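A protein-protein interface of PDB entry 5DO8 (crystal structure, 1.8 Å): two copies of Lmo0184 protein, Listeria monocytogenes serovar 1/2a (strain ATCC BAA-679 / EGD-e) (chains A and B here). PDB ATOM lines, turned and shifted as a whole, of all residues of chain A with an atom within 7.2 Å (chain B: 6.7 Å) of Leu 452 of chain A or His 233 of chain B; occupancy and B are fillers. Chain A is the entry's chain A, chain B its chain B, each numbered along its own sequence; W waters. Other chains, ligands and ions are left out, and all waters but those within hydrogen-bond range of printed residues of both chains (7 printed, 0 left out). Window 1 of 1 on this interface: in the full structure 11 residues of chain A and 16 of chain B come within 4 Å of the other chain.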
ATOM      1  N   TYR A  40     -12.536  -0.692  16.138  1.00  0.00           N
ATOM      2  CA  TYR A  40     -13.685  -1.469  16.618  1.00  0.00           C
ATOM      3  C   TYR A  40     -14.162  -2.452  15.538  1.00  0.00           C
ATOM      4  O   TYR A  40     -14.363  -3.635  15.800  1.00  0.00           O
ATOM      5  CB  TYR A  40     -14.852  -0.564  17.080  1.00  0.00           C
ATOM      6  CG  TYR A  40     -16.144  -1.340  17.183  1.00  0.00           C
ATOM      7  CD1 TYR A  40     -16.340  -2.249  18.219  1.00  0.00           C
ATOM      8  CD2 TYR A  40     -17.149  -1.193  16.231  1.00  0.00           C
ATOM      9  CE1 TYR A  40     -17.500  -2.998  18.302  1.00  0.00           C
ATOM     10  CE2 TYR A  40     -18.317  -1.939  16.302  1.00  0.00           C
ATOM     11  CZ  TYR A  40     -18.486  -2.843  17.349  1.00  0.00           C
ATOM     12  OH  TYR A  40     -19.637  -3.599  17.459  1.00  0.00           O
ATOM     13  N   GLU A  43     -11.786  -5.278  15.076  1.00  0.00           N
ATOM     14  CA  GLU A  43     -11.917  -6.186  16.230  1.00  0.00           C
ATOM     15  C   GLU A  43     -13.150  -7.108  16.130  1.00  0.00           C
ATOM     16  O   GLU A  43     -13.075  -8.279  16.465  1.00  0.00           O
ATOM     17  CB  GLU A  43     -11.950  -5.389  17.535  1.00  0.00           C
ATOM     18  CG  GLU A  43     -11.951  -6.277  18.777  1.00  0.00           C
ATOM     19  CD  GLU A  43     -11.559  -5.565  20.073  1.00  0.00           C
ATOM     20  OE1 GLU A  43     -11.840  -6.145  21.138  1.00  0.00           O
ATOM     21  OE2 GLU A  43     -10.943  -4.460  20.059  1.00  0.00           O
ATOM     22  N   ILE A 369     -25.136  -5.625  18.365  1.00  0.00           N
ATOM     23  CA  ILE A 369     -25.434  -5.342  19.772  1.00  0.00           C
ATOM     24  C   ILE A 369     -26.934  -5.474  20.049  1.00  0.00           C
ATOM     25  O   ILE A 369     -27.399  -5.123  21.139  1.00  0.00           O
ATOM     26  CB  ILE A 369     -24.894  -3.966  20.206  1.00  0.00           C
ATOM     27  CG1 ILE A 369     -25.546  -2.831  19.411  1.00  0.00           C
ATOM     28  CG2 ILE A 369     -23.387  -3.939  20.019  1.00  0.00           C
ATOM     29  CD1 ILE A 369     -25.392  -1.468  20.048  1.00  0.00           C
ATOM     30  N   TRP A 422     -23.781   3.790  21.218  1.00  0.00           N
ATOM     31  CA  TRP A 422     -22.390   3.536  21.615  1.00  0.00           C
ATOM     32  C   TRP A 422     -22.212   3.270  23.112  1.00  0.00           C
ATOM     33  O   TRP A 422     -21.437   2.389  23.494  1.00  0.00           O
ATOM     34  CB  TRP A 422     -21.461   4.685  21.175  1.00  0.00           C
ATOM     35  CG  TRP A 422     -21.308   4.682  19.715  1.00  0.00           C
ATOM     36  CD1 TRP A 422     -21.917   5.528  18.822  1.00  0.00           C
ATOM     37  CD2 TRP A 422     -20.536   3.757  18.935  1.00  0.00           C
ATOM     38  NE1 TRP A 422     -21.575   5.180  17.542  1.00  0.00           N
ATOM     39  CE2 TRP A 422     -20.733   4.099  17.575  1.00  0.00           C
ATOM     40  CE3 TRP A 422     -19.720   2.660  19.247  1.00  0.00           C
ATOM     41  CZ2 TRP A 422     -20.137   3.395  16.539  1.00  0.00           C
ATOM     42  CZ3 TRP A 422     -19.111   1.957  18.209  1.00  0.00           C
ATOM     43  CH2 TRP A 422     -19.328   2.322  16.871  1.00  0.00           C
ATOM     44  N   ASN A 447     -26.356  -1.054  24.417  1.00  0.00           N
ATOM     45  CA  ASN A 447     -25.318  -0.214  23.830  1.00  0.00           C
ATOM     46  C   ASN A 447     -24.022  -0.956  23.685  1.00  0.00           C
ATOM     47  O   ASN A 447     -23.821  -2.021  24.287  1.00  0.00           O
ATOM     48  CB  ASN A 447     -25.159   1.101  24.614  1.00  0.00           C
ATOM     49  CG  ASN A 447     -24.746   0.892  26.069  1.00  0.00           C
ATOM     50  OD1 ASN A 447     -23.590   0.586  26.349  1.00  0.00           O
ATOM     51  ND2 ASN A 447     -25.677   1.076  26.998  1.00  0.00           N
ATOM     52  N   ASN A 448     -23.140  -0.386  22.874  1.00  0.00           N
ATOM     53  CA  ASN A 448     -21.897  -1.041  22.492  1.00  0.00           C
ATOM     54  C   ASN A 448     -21.005  -1.288  23.710  1.00  0.00           C
ATOM     55  O   ASN A 448     -20.474  -2.394  23.878  1.00  0.00           O
ATOM     56  CB  ASN A 448     -21.225  -0.219  21.401  1.00  0.00           C
ATOM     57  CG  ASN A 448     -19.860  -0.742  20.981  1.00  0.00           C
ATOM     58  OD1 ASN A 448     -18.847  -0.532  21.654  1.00  0.00           O
ATOM     59  ND2 ASN A 448     -19.824  -1.369  19.838  1.00  0.00           N
ATOM     60  N   GLU A 449     -20.840  -0.272  24.554  1.00  0.00           N
ATOM     61  CA  GLU A 449     -20.036  -0.420  25.769  1.00  0.00           C
ATOM     62  C   GLU A 449     -20.499  -1.590  26.666  1.00  0.00           C
ATOM     63  O   GLU A 449     -19.659  -2.416  27.058  1.00  0.00           O
ATOM     64  CB  GLU A 449     -19.986   0.876  26.572  1.00  0.00           C
ATOM     65  CG  GLU A 449     -19.275   0.730  27.901  1.00  0.00           C
ATOM     66  CD  GLU A 449     -18.922   2.039  28.566  1.00  0.00           C
ATOM     67  OE1 GLU A 449     -18.567   1.998  29.758  1.00  0.00           O
ATOM     68  OE2 GLU A 449     -18.972   3.093  27.909  1.00  0.00           O
ATOM     69  N   GLU A 450     -21.798  -1.655  26.990  1.00  0.00           N
ATOM     70  CA  GLU A 450     -22.331  -2.772  27.794  1.00  0.00           C
ATOM     71  C   GLU A 450     -22.075  -4.113  27.095  1.00  0.00           C
ATOM     72  O   GLU A 450     -21.689  -5.087  27.744  1.00  0.00           O
ATOM     73  CB  GLU A 450     -23.841  -2.614  28.107  1.00  0.00           C
ATOM     74  CG  GLU A 450     -24.288  -3.123  29.491  1.00  0.00           C
ATOM     75  CD  GLU A 450     -25.001  -4.501  29.560  1.00  0.00           C
ATOM     76  OE1 GLU A 450     -26.245  -4.517  29.760  1.00  0.00           O
ATOM     77  OE2 GLU A 450     -24.358  -5.588  29.483  1.00  0.00           O
ATOM     78  N   ALA A 451     -22.255  -4.159  25.773  1.00  0.00           N
ATOM     79  CA  ALA A 451     -22.005  -5.381  25.019  1.00  0.00           C
ATOM     80  C   ALA A 451     -20.521  -5.795  25.075  1.00  0.00           C
ATOM     81  O   ALA A 451     -20.229  -6.966  25.294  1.00  0.00           O
ATOM     82  CB  ALA A 451     -22.461  -5.236  23.596  1.00  0.00           C
ATOM     83  N   LEU A 452     -19.595  -4.849  24.921  1.00  0.00           N
ATOM     84  CA  LEU A 452     -18.170  -5.186  25.031  1.00  0.00           C
ATOM     85  C   LEU A 452     -17.757  -5.651  26.447  1.00  0.00           C
ATOM     86  O   LEU A 452     -16.852  -6.491  26.595  1.00  0.00           O
ATOM     87  CB  LEU A 452     -17.285  -4.036  24.546  1.00  0.00           C
ATOM     88  CG  LEU A 452     -17.335  -3.783  23.044  1.00  0.00           C
ATOM     89  CD1 LEU A 452     -16.551  -2.532  22.664  1.00  0.00           C
ATOM     90  CD2 LEU A 452     -16.791  -4.954  22.273  1.00  0.00           C
ATOM     91  N   LYS A 453     -18.404  -5.119  27.471  1.00  0.00           N
ATOM     92  CA  LYS A 453     -18.094  -5.532  28.849  1.00  0.00           C
ATOM     93  C   LYS A 453     -18.647  -6.900  29.214  1.00  0.00           C
ATOM     94  O   LYS A 453     -18.126  -7.554  30.107  1.00  0.00           O
ATOM     95  CB  LYS A 453     -18.578  -4.492  29.852  1.00  0.00           C
ATOM     96  CG  LYS A 453     -17.757  -3.212  29.773  1.00  0.00           C
ATOM     97  CD  LYS A 453     -18.082  -2.230  30.877  1.00  0.00           C
ATOM     98  CE  LYS A 453     -19.472  -1.680  30.767  1.00  0.00           C
ATOM     99  NZ  LYS A 453     -19.653  -0.469  31.626  1.00  0.00           N
ATOM    100  N   ASN A 454     -19.731  -7.299  28.570  1.00  0.00           N
ATOM    101  CA  ASN A 454     -20.418  -8.548  28.881  1.00  0.00           C
ATOM    102  C   ASN A 454     -19.951  -9.695  27.959  1.00  0.00           C
ATOM    103  O   ASN A 454     -20.251  -9.682  26.766  1.00  0.00           O
ATOM    104  CB  ASN A 454     -21.908  -8.319  28.696  1.00  0.00           C
ATOM    105  CG  ASN A 454     -22.725  -9.582  28.851  1.00  0.00           C
ATOM    106  OD1 ASN A 454     -22.272 -10.581  29.413  1.00  0.00           O
ATOM    107  ND2 ASN A 454     -23.966  -9.535  28.354  1.00  0.00           N
ATOM    108  N   PRO A 455     -19.263 -10.712  28.498  1.00  0.00           N
ATOM    109  CA  PRO A 455     -18.787 -11.817  27.627  1.00  0.00           C
ATOM    110  C   PRO A 455     -19.894 -12.653  26.958  1.00  0.00           C
ATOM    111  O   PRO A 455     -19.639 -13.302  25.939  1.00  0.00           O
ATOM    112  CB  PRO A 455     -17.934 -12.678  28.571  1.00  0.00           C
ATOM    113  CG  PRO A 455     -18.413 -12.352  29.916  1.00  0.00           C
ATOM    114  CD  PRO A 455     -18.937 -10.951  29.905  1.00  0.00           C
ATOM    115  N   SER A 457     -22.529 -11.313  25.570  1.00  0.00           N
ATOM    116  CA  SER A 457     -23.267 -10.372  24.738  1.00  0.00           C
ATOM    117  C   SER A 457     -23.425 -10.887  23.324  1.00  0.00           C
ATOM    118  O   SER A 457     -22.709 -11.794  22.873  1.00  0.00           O
ATOM    119  CB  SER A 457     -22.574  -9.006  24.648  1.00  0.00           C
ATOM    120  OG  SER A 457     -21.387  -9.107  23.869  1.00  0.00           O
ATOM    121  N   PHE A 459     -22.493  -9.176  20.818  1.00  0.00           N
ATOM    122  CA  PHE A 459     -21.241  -8.805  20.130  1.00  0.00           C
ATOM    123  C   PHE A 459     -20.274  -9.976  20.010  1.00  0.00           C
ATOM    124  O   PHE A 459     -19.808 -10.305  18.908  1.00  0.00           O
ATOM    125  CB  PHE A 459     -20.556  -7.619  20.791  1.00  0.00           C
ATOM    126  CG  PHE A 459     -19.211  -7.344  20.222  1.00  0.00           C
ATOM    127  CD1 PHE A 459     -19.079  -6.601  19.059  1.00  0.00           C
ATOM    128  CD2 PHE A 459     -18.081  -7.913  20.789  1.00  0.00           C
ATOM    129  CE1 PHE A 459     -17.822  -6.370  18.499  1.00  0.00           C
ATOM    130  CE2 PHE A 459     -16.820  -7.702  20.223  1.00  0.00           C
ATOM    131  CZ  PHE A 459     -16.700  -6.943  19.067  1.00  0.00           C
ATOM    132  N   TYR A 460     -19.979 -10.633  21.127  1.00  0.00           N
ATOM    133  CA  TYR A 460     -19.010 -11.725  21.087  1.00  0.00           C
ATOM    134  C   TYR A 460     -19.542 -12.903  20.287  1.00  0.00           C
ATOM    135  O   TYR A 460     -18.766 -13.591  19.621  1.00  0.00           O
ATOM    136  CB  TYR A 460     -18.570 -12.122  22.493  1.00  0.00           C
ATOM    137  CG  TYR A 460     -17.777 -11.005  23.117  1.00  0.00           C
ATOM    138  CD1 TYR A 460     -16.542 -10.658  22.608  1.00  0.00           C
ATOM    139  CD2 TYR A 460     -18.285 -10.258  24.189  1.00  0.00           C
ATOM    140  CE1 TYR A 460     -15.819  -9.604  23.139  1.00  0.00           C
ATOM    141  CE2 TYR A 460     -17.569  -9.198  24.731  1.00  0.00           C
ATOM    142  CZ  TYR A 460     -16.325  -8.885  24.216  1.00  0.00           C
ATOM    143  OH  TYR A 460     -15.617  -7.840  24.746  1.00  0.00           O
ATOM    144  N   GLN A 463     -18.888 -11.890  16.686  1.00  0.00           N
ATOM    145  CA  GLN A 463     -17.439 -12.006  16.517  1.00  0.00           C
ATOM    146  C   GLN A 463     -17.017 -13.466  16.274  1.00  0.00           C
ATOM    147  O   GLN A 463     -16.190 -13.756  15.383  1.00  0.00           O
ATOM    148  CB  GLN A 463     -16.711 -11.464  17.751  1.00  0.00           C
ATOM    149  CG  GLN A 463     -15.218 -11.374  17.583  1.00  0.00           C
ATOM    150  CD  GLN A 463     -14.533 -10.974  18.873  1.00  0.00           C
ATOM    151  OE1 GLN A 463     -14.677 -11.651  19.895  1.00  0.00           O
ATOM    152  NE2 GLN A 463     -13.764  -9.877  18.833  1.00  0.00           N
ATOM    153  N   GLY B 229      -9.878 -11.156  24.394  1.00  0.00           N
ATOM    154  CA  GLY B 229     -10.934 -12.127  24.575  1.00  0.00           C
ATOM    155  C   GLY B 229     -12.142 -11.545  25.289  1.00  0.00           C
ATOM    156  O   GLY B 229     -12.077 -10.437  25.838  1.00  0.00           O
ATOM    157  N   PRO B 230     -13.244 -12.306  25.324  1.00  0.00           N
ATOM    158  CA  PRO B 230     -14.499 -11.768  25.832  1.00  0.00           C
ATOM    159  C   PRO B 230     -14.533 -11.413  27.312  1.00  0.00           C
ATOM    160  O   PRO B 230     -15.354 -10.591  27.695  1.00  0.00           O
ATOM    161  CB  PRO B 230     -15.508 -12.899  25.553  1.00  0.00           C
ATOM    162  CG  PRO B 230     -14.868 -13.738  24.512  1.00  0.00           C
ATOM    163  CD  PRO B 230     -13.412 -13.690  24.850  1.00  0.00           C
ATOM    164  N   ARG B 231     -13.665 -12.014  28.132  1.00  0.00           N
ATOM    165  CA  ARG B 231     -13.762 -11.916  29.591  1.00  0.00           C
ATOM    166  C   ARG B 231     -12.806 -10.904  30.249  1.00  0.00           C
ATOM    167  O   ARG B 231     -12.750 -10.823  31.477  1.00  0.00           O
ATOM    168  CB  ARG B 231     -13.519 -13.307  30.201  1.00  0.00           C
ATOM    169  CG  ARG B 231     -14.536 -14.338  29.730  1.00  0.00           C
ATOM    170  CD  ARG B 231     -14.403 -15.645  30.488  1.00  0.00           C
ATOM    171  NE  ARG B 231     -14.963 -15.540  31.845  1.00  0.00           N
ATOM    172  CZ  ARG B 231     -15.006 -16.536  32.722  1.00  0.00           C
ATOM    173  NH1 ARG B 231     -14.502 -17.734  32.420  1.00  0.00           N
ATOM    174  NH2 ARG B 231     -15.557 -16.344  33.910  1.00  0.00           N
ATOM    175  N   ILE B 232     -12.068 -10.126  29.464  1.00  0.00           N
ATOM    176  CA  ILE B 232     -11.077  -9.205  30.041  1.00  0.00           C
ATOM    177  C   ILE B 232     -11.764  -8.196  30.986  1.00  0.00           C
ATOM    178  O   ILE B 232     -11.341  -8.017  32.133  1.00  0.00           O
ATOM    179  CB  ILE B 232     -10.258  -8.445  28.976  1.00  0.00           C
ATOM    180  CG1 ILE B 232      -9.469  -9.395  28.080  1.00  0.00           C
ATOM    181  CG2 ILE B 232      -9.239  -7.536  29.639  1.00  0.00           C
ATOM    182  CD1 ILE B 232      -8.414 -10.175  28.841  1.00  0.00           C
ATOM    183  N   HIS B 233     -12.825  -7.544  30.504  1.00  0.00           N
ATOM    184  CA  HIS B 233     -13.545  -6.551  31.342  1.00  0.00           C
ATOM    185  C   HIS B 233     -14.082  -7.209  32.604  1.00  0.00           C
ATOM    186  O   HIS B 233     -13.950  -6.659  33.709  1.00  0.00           O
ATOM    187  CB  HIS B 233     -14.679  -5.858  30.577  1.00  0.00           C
ATOM    188  CG  HIS B 233     -14.203  -4.995  29.457  1.00  0.00           C
ATOM    189  ND1 HIS B 233     -13.475  -3.842  29.662  1.00  0.00           N
ATOM    190  CD2 HIS B 233     -14.317  -5.131  28.113  1.00  0.00           C
ATOM    191  CE1 HIS B 233     -13.176  -3.298  28.497  1.00  0.00           C
ATOM    192  NE2 HIS B 233     -13.673  -4.060  27.540  1.00  0.00           N
ATOM    193  N   GLU B 234     -14.681  -8.382  32.441  1.00  0.00           N
ATOM    194  CA  GLU B 234     -15.154  -9.172  33.573  1.00  0.00           C
ATOM    195  C   GLU B 234     -14.044  -9.391  34.600  1.00  0.00           C
ATOM    196  O   GLU B 234     -14.241  -9.168  35.795  1.00  0.00           O
ATOM    197  CB  GLU B 234     -15.692 -10.528  33.098  1.00  0.00           C
ATOM    198  CG  GLU B 234     -16.262 -11.395  34.210  1.00  0.00           C
ATOM    199  CD  GLU B 234     -16.407 -12.858  33.842  1.00  0.00           C
ATOM    200  OE1 GLU B 234     -16.400 -13.216  32.653  1.00  0.00           O
ATOM    201  OE2 GLU B 234     -16.510 -13.681  34.770  1.00  0.00           O
ATOM    202  N   PHE B 235     -12.890  -9.858  34.132  1.00  0.00           N
ATOM    203  CA  PHE B 235     -11.805 -10.208  35.043  1.00  0.00           C
ATOM    204  C   PHE B 235     -11.247  -8.969  35.735  1.00  0.00           C
ATOM    205  O   PHE B 235     -10.969  -8.988  36.933  1.00  0.00           O
ATOM    206  CB  PHE B 235     -10.690 -10.954  34.307  1.00  0.00           C
ATOM    207  CG  PHE B 235     -11.061 -12.343  33.834  1.00  0.00           C
ATOM    208  CD1 PHE B 235     -12.024 -13.129  34.481  1.00  0.00           C
ATOM    209  CD2 PHE B 235     -10.372 -12.903  32.750  1.00  0.00           C
ATOM    210  CE1 PHE B 235     -12.332 -14.404  34.021  1.00  0.00           C
ATOM    211  CE2 PHE B 235     -10.667 -14.183  32.308  1.00  0.00           C
ATOM    212  CZ  PHE B 235     -11.645 -14.934  32.943  1.00  0.00           C
ATOM    213  N   LEU B 236     -11.097  -7.888  34.982  1.00  0.00           N
ATOM    214  CA  LEU B 236     -10.623  -6.624  35.544  1.00  0.00           C
ATOM    215  C   LEU B 236     -11.570  -6.049  36.578  1.00  0.00           C
ATOM    216  O   LEU B 236     -11.115  -5.572  37.613  1.00  0.00           O
ATOM    217  CB  LEU B 236     -10.323  -5.596  34.451  1.00  0.00           C
ATOM    218  CG  LEU B 236      -9.097  -5.861  33.601  1.00  0.00           C
ATOM    219  CD1 LEU B 236      -8.986  -4.807  32.504  1.00  0.00           C
ATOM    220  CD2 LEU B 236      -7.840  -5.912  34.451  1.00  0.00           C
ATOM    221  N   GLN B 237     -12.882  -6.116  36.319  1.00  0.00           N
ATOM    222  CA  GLN B 237     -13.885  -5.679  37.308  1.00  0.00           C
ATOM    223  C   GLN B 237     -13.810  -6.527  38.565  1.00  0.00           C
ATOM    224  O   GLN B 237     -13.873  -6.001  39.666  1.00  0.00           O
ATOM    225  CB  GLN B 237     -15.318  -5.753  36.766  1.00  0.00           C
ATOM    226  CG  GLN B 237     -15.672  -4.691  35.742  1.00  0.00           C
ATOM    227  CD  GLN B 237     -16.900  -5.045  34.896  1.00  0.00           C
ATOM    228  OE1 GLN B 237     -17.693  -5.930  35.234  1.00  0.00           O
ATOM    229  NE2 GLN B 237     -17.033  -4.375  33.764  1.00  0.00           N
ATOM    230  N   GLU B 238     -13.704  -7.847  38.386  1.00  0.00           N
ATOM    231  CA  GLU B 238     -13.606  -8.797  39.515  1.00  0.00           C
ATOM    232  C   GLU B 238     -12.344  -8.531  40.352  1.00  0.00           C
ATOM    233  O   GLU B 238     -12.380  -8.517  41.591  1.00  0.00           O
ATOM    234  CB  GLU B 238     -13.639 -10.231  38.974  1.00  0.00           C
ATOM    235  CG  GLU B 238     -13.661 -11.342  39.998  1.00  0.00           C
ATOM    236  CD  GLU B 238     -13.484 -12.724  39.363  1.00  0.00           C
ATOM    237  OE1 GLU B 238     -12.363 -13.068  38.933  1.00  0.00           O
ATOM    238  OE2 GLU B 238     -14.475 -13.469  39.263  1.00  0.00           O
ATOM    239  N   THR B 261     -11.075   2.641  21.356  1.00  0.00           N
ATOM    240  CA  THR B 261     -12.451   2.288  21.788  1.00  0.00           C
ATOM    241  C   THR B 261     -12.459   1.447  23.054  1.00  0.00           C
ATOM    242  O   THR B 261     -13.130   1.771  24.044  1.00  0.00           O
ATOM    243  CB  THR B 261     -13.152   1.413  20.716  1.00  0.00           C
ATOM    244  OG1 THR B 261     -13.516   2.200  19.583  1.00  0.00           O
ATOM    245  CG2 THR B 261     -14.397   0.733  21.295  1.00  0.00           C
ATOM    246  N   ASP B 262     -11.684   0.370  23.023  1.00  0.00           N
ATOM    247  CA  ASP B 262     -11.560  -0.533  24.180  1.00  0.00           C
ATOM    248  C   ASP B 262     -10.969   0.212  25.383  1.00  0.00           C
ATOM    249  O   ASP B 262     -11.437   0.062  26.510  1.00  0.00           O
ATOM    250  CB  ASP B 262     -10.637  -1.716  23.896  1.00  0.00           C
ATOM    251  CG  ASP B 262     -11.097  -2.575  22.735  1.00  0.00           C
ATOM    252  OD1 ASP B 262     -12.311  -2.611  22.434  1.00  0.00           O
ATOM    253  OD2 ASP B 262     -10.201  -3.192  22.114  1.00  0.00           O
ATOM    254  N   ALA B 263      -9.932   1.006  25.141  1.00  0.00           N
ATOM    255  CA  ALA B 263      -9.302   1.750  26.228  1.00  0.00           C
ATOM    256  C   ALA B 263     -10.227   2.793  26.866  1.00  0.00           C
ATOM    257  O   ALA B 263     -10.129   3.058  28.057  1.00  0.00           O
ATOM    258  CB  ALA B 263      -8.015   2.382  25.733  1.00  0.00           C
ATOM    259  N   ILE B 265     -13.236   2.270  27.495  1.00  0.00           N
ATOM    260  CA  ILE B 265     -13.980   1.475  28.460  1.00  0.00           C
ATOM    261  C   ILE B 265     -13.113   1.141  29.671  1.00  0.00           C
ATOM    262  O   ILE B 265     -13.524   1.396  30.810  1.00  0.00           O
ATOM    263  CB  ILE B 265     -14.566   0.203  27.799  1.00  0.00           C
ATOM    264  CG1 ILE B 265     -15.501   0.593  26.648  1.00  0.00           C
ATOM    265  CG2 ILE B 265     -15.310  -0.648  28.830  1.00  0.00           C
ATOM    266  CD1 ILE B 265     -15.801  -0.546  25.692  1.00  0.00           C
ATOM    267  N   TYR B 266     -11.914   0.605  29.420  1.00  0.00           N
ATOM    268  CA  TYR B 266     -10.986   0.188  30.487  1.00  0.00           C
ATOM    269  C   TYR B 266     -10.661   1.309  31.454  1.00  0.00           C
ATOM    270  O   TYR B 266     -10.512   1.058  32.641  1.00  0.00           O
ATOM    271  CB  TYR B 266      -9.659  -0.313  29.909  1.00  0.00           C
ATOM    272  CG  TYR B 266      -9.738  -1.627  29.177  1.00  0.00           C
ATOM    273  CD1 TYR B 266     -10.213  -2.752  29.816  1.00  0.00           C
ATOM    274  CD2 TYR B 266      -9.301  -1.760  27.865  1.00  0.00           C
ATOM    275  CE1 TYR B 266     -10.266  -3.974  29.170  1.00  0.00           C
ATOM    276  CE2 TYR B 266      -9.377  -2.983  27.198  1.00  0.00           C
ATOM    277  CZ  TYR B 266      -9.857  -4.079  27.862  1.00  0.00           C
ATOM    278  OH  TYR B 266      -9.932  -5.304  27.231  1.00  0.00           O
ATOM    279  N   ASN B 271     -16.271   2.456  35.266  1.00  0.00           N
ATOM    280  CA  ASN B 271     -16.193   1.029  35.043  1.00  0.00           C
ATOM    281  C   ASN B 271     -15.329   0.271  36.039  1.00  0.00           C
ATOM    282  O   ASN B 271     -15.381  -0.952  36.060  1.00  0.00           O
ATOM    283  CB  ASN B 271     -15.753   0.753  33.614  1.00  0.00           C
ATOM    284  CG  ASN B 271     -16.758   1.267  32.613  1.00  0.00           C
ATOM    285  OD1 ASN B 271     -17.959   1.285  32.900  1.00  0.00           O
ATOM    286  ND2 ASN B 271     -16.293   1.693  31.454  1.00  0.00           N
ATOM    287  N   ASN B 272     -14.555   0.990  36.845  1.00  0.00           N
ATOM    288  CA  ASN B 272     -13.740   0.384  37.907  1.00  0.00           C
ATOM    289  C   ASN B 272     -12.891  -0.759  37.365  1.00  0.00           C
ATOM    290  O   ASN B 272     -12.973  -1.907  37.830  1.00  0.00           O
ATOM    291  CB  ASN B 272     -14.636  -0.086  39.061  1.00  0.00           C
ATOM    292  CG  ASN B 272     -15.381   1.057  39.719  1.00  0.00           C
ATOM    293  OD1 ASN B 272     -14.802   2.076  40.059  1.00  0.00           O
ATOM    294  ND2 ASN B 272     -16.679   0.885  39.895  1.00  0.00           N
ATOM    295  N   GLU B 273     -12.123  -0.459  36.318  1.00  0.00           N
ATOM    296  CA  GLU B 273     -11.219  -1.439  35.747  1.00  0.00           C
ATOM    297  C   GLU B 273      -9.796  -0.961  36.040  1.00  0.00           C
ATOM    298  O   GLU B 273      -9.267  -1.286  37.111  1.00  0.00           O
ATOM    299  CB  GLU B 273     -11.581  -1.720  34.282  1.00  0.00           C
ATOM    300  CG  GLU B 273     -12.963  -2.392  34.194  1.00  0.00           C
ATOM    301  CD  GLU B 273     -13.433  -2.728  32.802  1.00  0.00           C
ATOM    302  OE1 GLU B 273     -12.598  -2.812  31.893  1.00  0.00           O
ATOM    303  OE2 GLU B 273     -14.662  -2.941  32.605  1.00  0.00           O
HETATM  304  O   HOH W   1     -19.130  -1.557  34.213  1.00  0.00           O
HETATM  305  O   HOH W   2     -12.141  -2.136  19.337  1.00  0.00           O
HETATM  306  O   HOH W   3     -11.791  -5.704  23.843  1.00  0.00           O
HETATM  307  O   HOH W   4     -18.601  -7.996  32.768  1.00  0.00           O
HETATM  308  O   HOH W   5     -12.109   2.030  17.170  1.00  0.00           O
HETATM  309  O   HOH W   6     -12.811  -7.890  25.010  1.00  0.00           O
HETATM  310  O   HOH W   7     -15.755  -9.103  29.922  1.00  0.00           O
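Of the 17 printed residues of chain A, 7 touch a printed residue of chain B. Among the printed residues, 15 pairs touch across the chains. Among the printed residues, no Asp or Glu carboxylate lies within 4 Å of a Lys or Arg side-chain nitrogen of the other chain.
Tyr 40 of chain A touches Thr 261 of chain B. His 233 of chain B touches Leu 452 of chain A (CD2 to O, 3.3 Å). His 233 of chain B touches Lys 453 of chain A (CB to CA, 3.8 Å). Lys 453 of chain A touches Gln 237 of chain B (CD to NE2, 3.7 Å). Lys 453 of chain A touches Glu 273 of chain B (CD to OE2, 3.9 Å). Pro 455 of chain A touches Arg 231 of chain B (CB to CG, 3.96 Å). Glu 234 of chain B touches Pro 455 of chain A. CA of Pro 230 of chain B touches CE1 of Tyr 460 of chain A, 3.7 Å away.
Water W2 lies within hydrogen-bond range of OE2 of Glu 43 of chain A (2.7 Å) and OD1 of Asp 262 of chain B (3.1 Å). Water W6 bridges the backbone carbonyl oxygen of Gly 229 of chain B (2.8 Å) and the side-chain hydroxyl of Tyr 460 of chain A (2.8 Å). Water W5 bridges the side-chain hydroxyl (OG1) of Thr 261 of chain B (2.8 Å) and the backbone NH (N) of Tyr 40 of chain A (2.9 Å).
The side-chain hydroxyl (OG) of Ser 457 of chain A lies close to the backbone NH (N) of Tyr 460 of chain A. O of Ile 265 of chain B is in hydrogen-bond range of ND2 of Asn 271 of chain B, 2.9 Å away. NE2 of Gln 463 of chain A sits at hydrogen-bond distance from O of Glu 43 of chain A (2.9 Å). OE2 of Glu 273 of chain B lies within hydrogen-bond range of NE2 of Gln 237 of chain B (3.0 Å). OE1 of Glu 273 of chain B sits at hydrogen-bond distance from ND1 of His 233 of chain B, 2.6 Å away.
The side-chain carboxylate (OD2) of Asp 262 of chain B lies close to the side-chain carboxylate (OE2) of Glu 43 of chain A, 2.5 Å away. The side-chain amide nitrogen of Asn 271 of chain B is in hydrogen-bond range of the side-chain carboxylate of Glu 449 of chain A (2.9 Å). The side-chain amino group (NZ) of Lys 453 of chain A sits at hydrogen-bond distance from the side-chain amide oxygen (OD1) of Asn 271 of chain B, 2.8 Å away.
No position is printed for both chains. Of the 15 pairs that touch across the chains among the printed residues, none has its exchanged pair printed and touching as well.
Leu 452 of chain A touches just these residues of chain B: His 233 and Ile 265. Of the printed residues of chain B, Glu 449 of chain A touches Ile 265 and Asn 271. Of the printed residues of chain B, Pro 455 of chain A touches Pro 230 (3.4 Å), Arg 231 (3.96 Å) and Glu 234 (3.5 Å). Ile 232 of chain B touches none of the printed residues of chain A. The nearest printed residue of chain B that does not touch Leu 452 of chain A is Thr 261 of chain B (4.1 Å). The nearest residue of chain A that does not touch His 233 of chain B is Tyr 460 of chain A (4.5 Å). The nearest printed residue of chain A that does not touch Glu 273 of chain B is Glu 449 of chain A (6.9 Å).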
